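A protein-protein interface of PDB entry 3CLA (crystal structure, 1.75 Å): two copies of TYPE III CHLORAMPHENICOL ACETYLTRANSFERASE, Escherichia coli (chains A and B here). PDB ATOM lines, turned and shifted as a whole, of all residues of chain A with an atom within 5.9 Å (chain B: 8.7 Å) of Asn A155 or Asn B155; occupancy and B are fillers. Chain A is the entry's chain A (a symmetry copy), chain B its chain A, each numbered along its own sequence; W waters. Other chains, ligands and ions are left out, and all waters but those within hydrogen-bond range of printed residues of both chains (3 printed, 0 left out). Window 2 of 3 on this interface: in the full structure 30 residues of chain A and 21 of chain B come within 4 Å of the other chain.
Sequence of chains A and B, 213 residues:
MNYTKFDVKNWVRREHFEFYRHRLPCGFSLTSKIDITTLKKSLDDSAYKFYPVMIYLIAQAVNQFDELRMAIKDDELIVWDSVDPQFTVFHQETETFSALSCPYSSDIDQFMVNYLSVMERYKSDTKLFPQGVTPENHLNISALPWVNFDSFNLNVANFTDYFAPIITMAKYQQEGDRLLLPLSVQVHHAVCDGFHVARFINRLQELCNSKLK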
ATOM      1  N   PRO A  25     -30.495  33.028 -30.968  1.00  0.00           N
ATOM      2  CA  PRO A  25     -29.166  32.441 -31.320  1.00  0.00           C
ATOM      3  C   PRO A  25     -28.474  31.932 -30.048  1.00  0.00           C
ATOM      4  O   PRO A  25     -28.382  32.693 -29.048  1.00  0.00           O
ATOM      5  CB  PRO A  25     -28.394  33.597 -31.922  1.00  0.00           C
ATOM      6  CG  PRO A  25     -29.442  34.634 -32.281  1.00  0.00           C
ATOM      7  CD  PRO A  25     -30.553  34.460 -31.271  1.00  0.00           C
ATOM      8  N   CYS A  26     -28.051  30.680 -30.094  1.00  0.00           N
ATOM      9  CA  CYS A  26     -27.356  30.135 -28.933  1.00  0.00           C
ATOM     10  C   CYS A  26     -26.679  28.802 -29.375  1.00  0.00           C
ATOM     11  O   CYS A  26     -26.979  28.222 -30.429  1.00  0.00           O
ATOM     12  CB  CYS A  26     -28.262  29.864 -27.760  1.00  0.00           C
ATOM     13  SG  CYS A  26     -29.502  28.580 -28.028  1.00  0.00           S
ATOM     14  N   GLY A  27     -25.766  28.503 -28.469  1.00  0.00           N
ATOM     15  CA  GLY A  27     -24.997  27.245 -28.590  1.00  0.00           C
ATOM     16  C   GLY A  27     -24.892  26.693 -27.144  1.00  0.00           C
ATOM     17  O   GLY A  27     -25.351  27.338 -26.177  1.00  0.00           O
ATOM     18  N   PHE A  28     -24.264  25.558 -27.000  1.00  0.00           N
ATOM     19  CA  PHE A  28     -24.119  25.029 -25.620  1.00  0.00           C
ATOM     20  C   PHE A  28     -22.796  24.234 -25.641  1.00  0.00           C
ATOM     21  O   PHE A  28     -22.358  23.809 -26.710  1.00  0.00           O
ATOM     22  CB  PHE A  28     -25.338  24.198 -25.196  1.00  0.00           C
ATOM     23  CG  PHE A  28     -25.684  23.013 -26.084  1.00  0.00           C
ATOM     24  CD1 PHE A  28     -25.115  21.777 -25.780  1.00  0.00           C
ATOM     25  CD2 PHE A  28     -26.573  23.124 -27.157  1.00  0.00           C
ATOM     26  CE1 PHE A  28     -25.364  20.635 -26.569  1.00  0.00           C
ATOM     27  CE2 PHE A  28     -26.878  22.004 -27.948  1.00  0.00           C
ATOM     28  CZ  PHE A  28     -26.285  20.755 -27.631  1.00  0.00           C
ATOM     29  N   SER A  29     -22.337  24.026 -24.422  1.00  0.00           N
ATOM     30  CA  SER A  29     -21.168  23.138 -24.228  1.00  0.00           C
ATOM     31  C   SER A  29     -21.599  22.113 -23.148  1.00  0.00           C
ATOM     32  O   SER A  29     -22.519  22.380 -22.343  1.00  0.00           O
ATOM     33  CB  SER A  29     -19.884  23.832 -23.805  1.00  0.00           C
ATOM     34  OG  SER A  29     -20.137  24.437 -22.503  1.00  0.00           O
ATOM     35  N   ASN A 153     -15.606  25.727 -20.810  1.00  0.00           N
ATOM     36  CA  ASN A 153     -16.604  26.384 -21.738  1.00  0.00           C
ATOM     37  C   ASN A 153     -15.871  27.548 -22.367  1.00  0.00           C
ATOM     38  O   ASN A 153     -15.153  28.258 -21.611  1.00  0.00           O
ATOM     39  CB  ASN A 153     -17.810  26.862 -20.890  1.00  0.00           C
ATOM     40  CG  ASN A 153     -18.837  27.607 -21.723  1.00  0.00           C
ATOM     41  OD1 ASN A 153     -18.899  28.883 -21.717  1.00  0.00           O
ATOM     42  ND2 ASN A 153     -19.516  26.937 -22.617  1.00  0.00           N
ATOM     43  N   LEU A 154     -16.147  27.806 -23.652  1.00  0.00           N
ATOM     44  CA  LEU A 154     -15.543  28.990 -24.325  1.00  0.00           C
ATOM     45  C   LEU A 154     -16.618  30.108 -24.341  1.00  0.00           C
ATOM     46  O   LEU A 154     -17.707  29.747 -24.833  1.00  0.00           O
ATOM     47  CB  LEU A 154     -15.188  28.650 -25.794  1.00  0.00           C
ATOM     48  CG  LEU A 154     -13.838  27.913 -25.846  1.00  0.00           C
ATOM     49  CD1 LEU A 154     -13.861  27.075 -27.125  1.00  0.00           C
ATOM     50  CD2 LEU A 154     -12.730  28.979 -25.837  1.00  0.00           C
ATOM     51  N   ASN A 155     -16.278  31.268 -23.871  1.00  0.00           N
ATOM     52  CA  ASN A 155     -17.184  32.455 -23.890  1.00  0.00           C
ATOM     53  C   ASN A 155     -16.681  33.264 -25.101  1.00  0.00           C
ATOM     54  O   ASN A 155     -15.633  33.877 -25.065  1.00  0.00           O
ATOM     55  CB  ASN A 155     -17.055  33.168 -22.565  1.00  0.00           C
ATOM     56  CG  ASN A 155     -17.511  32.269 -21.413  1.00  0.00           C
ATOM     57  OD1 ASN A 155     -16.715  32.063 -20.456  1.00  0.00           O
ATOM     58  ND2 ASN A 155     -18.724  31.784 -21.444  1.00  0.00           N
ATOM     59  N   VAL A 156     -17.455  33.178 -26.181  1.00  0.00           N
ATOM     60  CA  VAL A 156     -17.090  33.850 -27.476  1.00  0.00           C
ATOM     61  C   VAL A 156     -18.011  35.046 -27.684  1.00  0.00           C
ATOM     62  O   VAL A 156     -19.257  34.846 -27.639  1.00  0.00           O
ATOM     63  CB  VAL A 156     -17.247  32.843 -28.633  1.00  0.00           C
ATOM     64  CG1 VAL A 156     -16.968  33.459 -29.979  1.00  0.00           C
ATOM     65  CG2 VAL A 156     -16.339  31.611 -28.445  1.00  0.00           C
ATOM     66  N   ALA A 157     -17.435  36.200 -27.892  1.00  0.00           N
ATOM     67  CA  ALA A 157     -18.163  37.452 -28.091  1.00  0.00           C
ATOM     68  C   ALA A 157     -19.048  37.395 -29.325  1.00  0.00           C
ATOM     69  O   ALA A 157     -20.131  37.980 -29.226  1.00  0.00           O
ATOM     70  CB  ALA A 157     -17.257  38.654 -28.112  1.00  0.00           C
ATOM     71  N   PHE A 159     -20.512  34.413 -32.291  1.00  0.00           N
ATOM     72  CA  PHE A 159     -20.345  33.025 -32.938  1.00  0.00           C
ATOM     73  C   PHE A 159     -21.382  32.903 -34.059  1.00  0.00           C
ATOM     74  O   PHE A 159     -21.826  31.771 -34.421  1.00  0.00           O
ATOM     75  CB  PHE A 159     -20.519  31.905 -31.900  1.00  0.00           C
ATOM     76  CG  PHE A 159     -21.747  32.011 -31.038  1.00  0.00           C
ATOM     77  CD1 PHE A 159     -22.953  31.420 -31.423  1.00  0.00           C
ATOM     78  CD2 PHE A 159     -21.711  32.702 -29.814  1.00  0.00           C
ATOM     79  CE1 PHE A 159     -24.133  31.497 -30.688  1.00  0.00           C
ATOM     80  CE2 PHE A 159     -22.884  32.815 -29.016  1.00  0.00           C
ATOM     81  CZ  PHE A 159     -24.071  32.195 -29.464  1.00  0.00           C
ATOM     82  N   GLN A 186     -18.521  21.696 -27.760  1.00  0.00           N
ATOM     83  CA  GLN A 186     -19.250  22.974 -27.819  1.00  0.00           C
ATOM     84  C   GLN A 186     -19.753  23.152 -29.255  1.00  0.00           C
ATOM     85  O   GLN A 186     -19.040  22.997 -30.244  1.00  0.00           O
ATOM     86  CB  GLN A 186     -18.285  24.091 -27.400  1.00  0.00           C
ATOM     87  CG  GLN A 186     -18.979  25.444 -27.367  1.00  0.00           C
ATOM     88  CD  GLN A 186     -18.354  26.428 -26.364  1.00  0.00           C
ATOM     89  OE1 GLN A 186     -17.674  26.065 -25.442  1.00  0.00           O
ATOM     90  NE2 GLN A 186     -18.565  27.698 -26.693  1.00  0.00           N
ATOM     91  N   GLY B  27     -25.097  36.468 -16.191  1.00  0.00           N
ATOM     92  CA  GLY B  27     -25.820  35.329 -15.584  1.00  0.00           C
ATOM     93  C   GLY B  27     -24.732  34.257 -15.312  1.00  0.00           C
ATOM     94  O   GLY B  27     -23.547  34.443 -15.662  1.00  0.00           O
ATOM     95  N   SER B  29     -24.089  29.743 -14.799  1.00  0.00           N
ATOM     96  CA  SER B  29     -24.636  28.368 -14.748  1.00  0.00           C
ATOM     97  C   SER B  29     -23.730  27.597 -13.755  1.00  0.00           C
ATOM     98  O   SER B  29     -22.563  27.983 -13.520  1.00  0.00           O
ATOM     99  CB  SER B  29     -24.688  27.637 -16.081  1.00  0.00           C
ATOM    100  OG  SER B  29     -23.312  27.496 -16.542  1.00  0.00           O
ATOM    101  N   PHE B 152     -22.846  21.606 -18.079  1.00  0.00           N
ATOM    102  CA  PHE B 152     -23.627  21.966 -19.261  1.00  0.00           C
ATOM    103  C   PHE B 152     -23.747  23.518 -19.204  1.00  0.00           C
ATOM    104  O   PHE B 152     -24.080  24.011 -18.080  1.00  0.00           O
ATOM    105  CB  PHE B 152     -25.078  21.312 -19.150  1.00  0.00           C
ATOM    106  CG  PHE B 152     -25.915  21.633 -20.377  1.00  0.00           C
ATOM    107  CD1 PHE B 152     -25.818  20.839 -21.560  1.00  0.00           C
ATOM    108  CD2 PHE B 152     -26.774  22.751 -20.352  1.00  0.00           C
ATOM    109  CE1 PHE B 152     -26.560  21.142 -22.710  1.00  0.00           C
ATOM    110  CE2 PHE B 152     -27.502  23.092 -21.502  1.00  0.00           C
ATOM    111  CZ  PHE B 152     -27.375  22.300 -22.673  1.00  0.00           C
ATOM    112  N   ASN B 153     -23.577  24.207 -20.306  1.00  0.00           N
ATOM    113  CA  ASN B 153     -23.795  25.701 -20.203  1.00  0.00           C
ATOM    114  C   ASN B 153     -24.413  26.115 -21.520  1.00  0.00           C
ATOM    115  O   ASN B 153     -23.921  25.623 -22.572  1.00  0.00           O
ATOM    116  CB  ASN B 153     -22.418  26.376 -19.983  1.00  0.00           C
ATOM    117  CG  ASN B 153     -22.520  27.889 -19.943  1.00  0.00           C
ATOM    118  OD1 ASN B 153     -22.208  28.604 -20.954  1.00  0.00           O
ATOM    119  ND2 ASN B 153     -23.141  28.443 -18.935  1.00  0.00           N
ATOM    120  N   LEU B 154     -25.350  27.070 -21.467  1.00  0.00           N
ATOM    121  CA  LEU B 154     -25.943  27.607 -22.724  1.00  0.00           C
ATOM    122  C   LEU B 154     -25.235  28.952 -23.031  1.00  0.00           C
ATOM    123  O   LEU B 154     -25.256  29.757 -22.078  1.00  0.00           O
ATOM    124  CB  LEU B 154     -27.452  27.900 -22.523  1.00  0.00           C
ATOM    125  CG  LEU B 154     -28.259  26.598 -22.680  1.00  0.00           C
ATOM    126  CD1 LEU B 154     -29.542  26.797 -21.872  1.00  0.00           C
ATOM    127  CD2 LEU B 154     -28.511  26.389 -24.181  1.00  0.00           C
ATOM    128  N   ASN B 155     -24.724  29.100 -24.214  1.00  0.00           N
ATOM    129  CA  ASN B 155     -24.077  30.366 -24.673  1.00  0.00           C
ATOM    130  C   ASN B 155     -25.176  31.037 -25.520  1.00  0.00           C
ATOM    131  O   ASN B 155     -25.477  30.616 -26.619  1.00  0.00           O
ATOM    132  CB  ASN B 155     -22.829  30.005 -25.441  1.00  0.00           C
ATOM    133  CG  ASN B 155     -21.822  29.283 -24.543  1.00  0.00           C
ATOM    134  OD1 ASN B 155     -21.390  28.154 -24.904  1.00  0.00           O
ATOM    135  ND2 ASN B 155     -21.414  29.884 -23.455  1.00  0.00           N
ATOM    136  N   VAL B 156     -25.787  32.056 -24.921  1.00  0.00           N
ATOM    137  CA  VAL B 156     -26.927  32.792 -25.569  1.00  0.00           C
ATOM    138  C   VAL B 156     -26.437  34.165 -26.012  1.00  0.00           C
ATOM    139  O   VAL B 156     -25.886  34.901 -25.146  1.00  0.00           O
ATOM    140  CB  VAL B 156     -28.083  32.934 -24.558  1.00  0.00           C
ATOM    141  CG1 VAL B 156     -29.242  33.724 -25.109  1.00  0.00           C
ATOM    142  CG2 VAL B 156     -28.593  31.560 -24.079  1.00  0.00           C
ATOM    143  N   ALA B 157     -26.621  34.476 -27.267  1.00  0.00           N
ATOM    144  CA  ALA B 157     -26.196  35.740 -27.865  1.00  0.00           C
ATOM    145  C   ALA B 157     -26.886  36.929 -27.214  1.00  0.00           C
ATOM    146  O   ALA B 157     -26.190  37.941 -27.089  1.00  0.00           O
ATOM    147  CB  ALA B 157     -26.354  35.759 -29.362  1.00  0.00           C
ATOM    148  N   ASN B 158     -28.100  36.873 -26.753  1.00  0.00           N
ATOM    149  CA  ASN B 158     -28.773  37.980 -26.027  1.00  0.00           C
ATOM    150  C   ASN B 158     -29.688  37.462 -24.940  1.00  0.00           C
ATOM    151  O   ASN B 158     -30.684  36.678 -25.236  1.00  0.00           O
ATOM    152  CB  ASN B 158     -29.556  38.781 -27.138  1.00  0.00           C
ATOM    153  N   PHE B 159     -29.462  37.817 -23.691  1.00  0.00           N
ATOM    154  CA  PHE B 159     -30.401  37.284 -22.594  1.00  0.00           C
ATOM    155  C   PHE B 159     -30.941  38.487 -21.813  1.00  0.00           C
ATOM    156  O   PHE B 159     -31.304  38.373 -20.603  1.00  0.00           O
ATOM    157  CB  PHE B 159     -29.668  36.304 -21.665  1.00  0.00           C
ATOM    158  CG  PHE B 159     -28.350  36.791 -21.128  1.00  0.00           C
ATOM    159  CD1 PHE B 159     -28.276  37.503 -19.928  1.00  0.00           C
ATOM    160  CD2 PHE B 159     -27.152  36.533 -21.817  1.00  0.00           C
ATOM    161  CE1 PHE B 159     -27.095  38.003 -19.385  1.00  0.00           C
ATOM    162  CE2 PHE B 159     -25.912  37.017 -21.312  1.00  0.00           C
ATOM    163  CZ  PHE B 159     -25.909  37.731 -20.095  1.00  0.00           C
ATOM    164  N   ILE B 166     -33.257  28.228 -16.178  1.00  0.00           N
ATOM    165  CA  ILE B 166     -33.143  27.180 -17.202  1.00  0.00           C
ATOM    166  C   ILE B 166     -32.558  25.968 -16.508  1.00  0.00           C
ATOM    167  O   ILE B 166     -31.471  26.129 -15.905  1.00  0.00           O
ATOM    168  CB  ILE B 166     -32.305  27.633 -18.440  1.00  0.00           C
ATOM    169  CG1 ILE B 166     -32.952  28.930 -19.029  1.00  0.00           C
ATOM    170  CG2 ILE B 166     -32.257  26.479 -19.505  1.00  0.00           C
ATOM    171  CD1 ILE B 166     -31.901  29.695 -19.943  1.00  0.00           C
ATOM    172  N   GLN B 186     -29.196  27.496 -14.769  1.00  0.00           N
ATOM    173  CA  GLN B 186     -28.643  28.706 -15.400  1.00  0.00           C
ATOM    174  C   GLN B 186     -29.627  29.851 -15.141  1.00  0.00           C
ATOM    175  O   GLN B 186     -30.837  29.758 -15.335  1.00  0.00           O
ATOM    176  CB  GLN B 186     -28.465  28.422 -16.897  1.00  0.00           C
ATOM    177  CG  GLN B 186     -27.831  29.603 -17.616  1.00  0.00           C
ATOM    178  CD  GLN B 186     -27.023  29.200 -18.861  1.00  0.00           C
ATOM    179  OE1 GLN B 186     -26.605  28.085 -19.026  1.00  0.00           O
ATOM    180  NE2 GLN B 186     -26.937  30.178 -19.756  1.00  0.00           N
HETATM  181  O   HOH W   1     -21.752  27.301 -27.841  1.00  0.00           O
HETATM  182  O   HOH W   2     -29.769  34.918 -28.137  1.00  0.00           O
HETATM  183  O   HOH W   3     -21.198  32.686 -22.690  1.00  0.00           O
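The backbone NH (N) of Ser A29 is in hydrogen-bond range of the backbone carbonyl oxygen (O) of Asn B153, at 2.9 Å. OD1 of Asn B153 sits close to OD1 of Asn A153, 3.4 Å away. The backbone carbonyl oxygen (O) of Gly A27 lies within hydrogen-bond range of the backbone NH (N) of Asn B155. The side-chain amide nitrogen (ND2) of Asn A153 is in hydrogen-bond range of the side-chain amide oxygen (OD1) of Asn B155 (3.2 Å). OD1 of Asn B155 sits at hydrogen-bond distance from NE2 of Gln A186 (3.4 Å). The backbone NH (N) of Ala B157 sits at hydrogen-bond distance from the backbone carbonyl oxygen (O) of Pro A25 (3.1 Å).
ND2 of Asn B153 is in hydrogen-bond range of OG of Ser B29, 2.6 Å away. The side-chain amide nitrogen of Asn B153 lies within hydrogen-bond range of the side-chain amide oxygen of Gln B186 (3.5 Å). The backbone carbonyl oxygen (O) of Leu B154 sits at hydrogen-bond distance from the side-chain amide nitrogen (NE2) of Gln B186 (2.9 Å). ND2 of Asn A153 is in hydrogen-bond range of OG of Ser A29 (2.6 Å). The side-chain amide nitrogen (ND2) of Asn A155 lies within hydrogen-bond range of the side-chain amide oxygen (OD1) of Asn A153 (2.9 Å). The side-chain amide nitrogen of Gln A186 is in hydrogen-bond range of the backbone carbonyl oxygen of Leu A154 (2.9 Å).
Among the printed residues, pairs that only touch across the chains: Pro A25 with Val B156 (3.8 Å), Cys A26 with Asn B155 (3.0 Å), Cys A26 with Val B156 (3.9 Å), Gly A27 with Leu B154 (3.5 Å), Phe A28 with Phe B152 (3.5 Å), Phe A28 with Asn B153 (3.1 Å), Phe A28 with Leu B154 (3.99 Å), Ser A29 with Phe B152 (3.3 Å), Leu A154 with Asn B155 (3.96 Å), Asn A155 with Asn B155 (3.9 Å) and Phe A159 with Asn B155 (3.5 Å).
Asn A155 touches one residue of chain B. Of the printed residues of chain A, Asn B155 touches Cys A26, Gly A27, Asn A153, Leu A154, Asn A155, Phe A159 and Gln A186. Of chain B, only Leu B154 and Asn B155 come within 4 Å of Gly A27. Of the printed residues of chain A, Phe B152 touches Phe A28 (3.5 Å) and Ser A29 (3.3 Å). Of the printed residues of chain B, Phe A159 touches Asn B155 (3.5 Å). Of the printed residues of chain B, Ser A29 touches Phe B152 (3.3 Å) and Asn B153 (2.9 Å). Printed residues of chain A within 4 Å of Ala B157: Pro A25. Printed residues of chain B within 4 Å of Pro A25: Val B156 (3.8 Å) and Ala B157 (3.1 Å). Gln B186 touches none of the printed residues of chain A. Asn B158 touches none of the printed residues of chain A. The nearest residue of chain A that does not touch Asn B155 is Phe A28 (4.2 Å).
Printed residues of chain A that touch a printed residue of chain B: Pro A25, Cys A26, Gly A27, Phe A28, Ser A29, Asn A153, Leu A154, Asn A155, Phe A159 and Gln A186. Among the printed residues, 17 pairs touch across the chains. Among the printed residues, no Asp or Glu carboxylate lies within 4 Å of a Lys or Arg side-chain nitrogen of the other chain.
Gly A27 touches Leu B154, but with the chains exchanged Leu A154 does not touch Gly B27 (11.8 Å). Gly A27 touches Asn B155, but with the chains exchanged Asn A155 does not touch Gly B27 (8.0 Å). Asn A153 touches its own counterpart, Asn B153. Asn A153 touches Asn B155, but with the chains exchanged Asn A155 does not touch Asn B153 (4.7 Å). Positions printed for both chains: 27, 29, 153, 154, 155, 156, 157, 159 and 186. Of the 17 pairs that touch across the chains among the printed residues, 2 have their exchanged pair printed and touching as well.
Water W2 lies within hydrogen-bond range of O of Pro A25 (2.8 Å), N of Asn B158 (2.9 Å) and N of Ala B157 (3.3 Å). Water W3 lies within hydrogen-bond range of ND2 of Asn B155 (2.9 Å) and ND2 of Asn A155 (2.9 Å). Water W1 lies within hydrogen-bond range of the side-chain amide oxygen (OD1) of Asn B155 (3.1 Å), the backbone NH (N) of Phe A28 (3.2 Å) and the side-chain amide nitrogen (NE2) of Gln A186 (3.4 Å).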
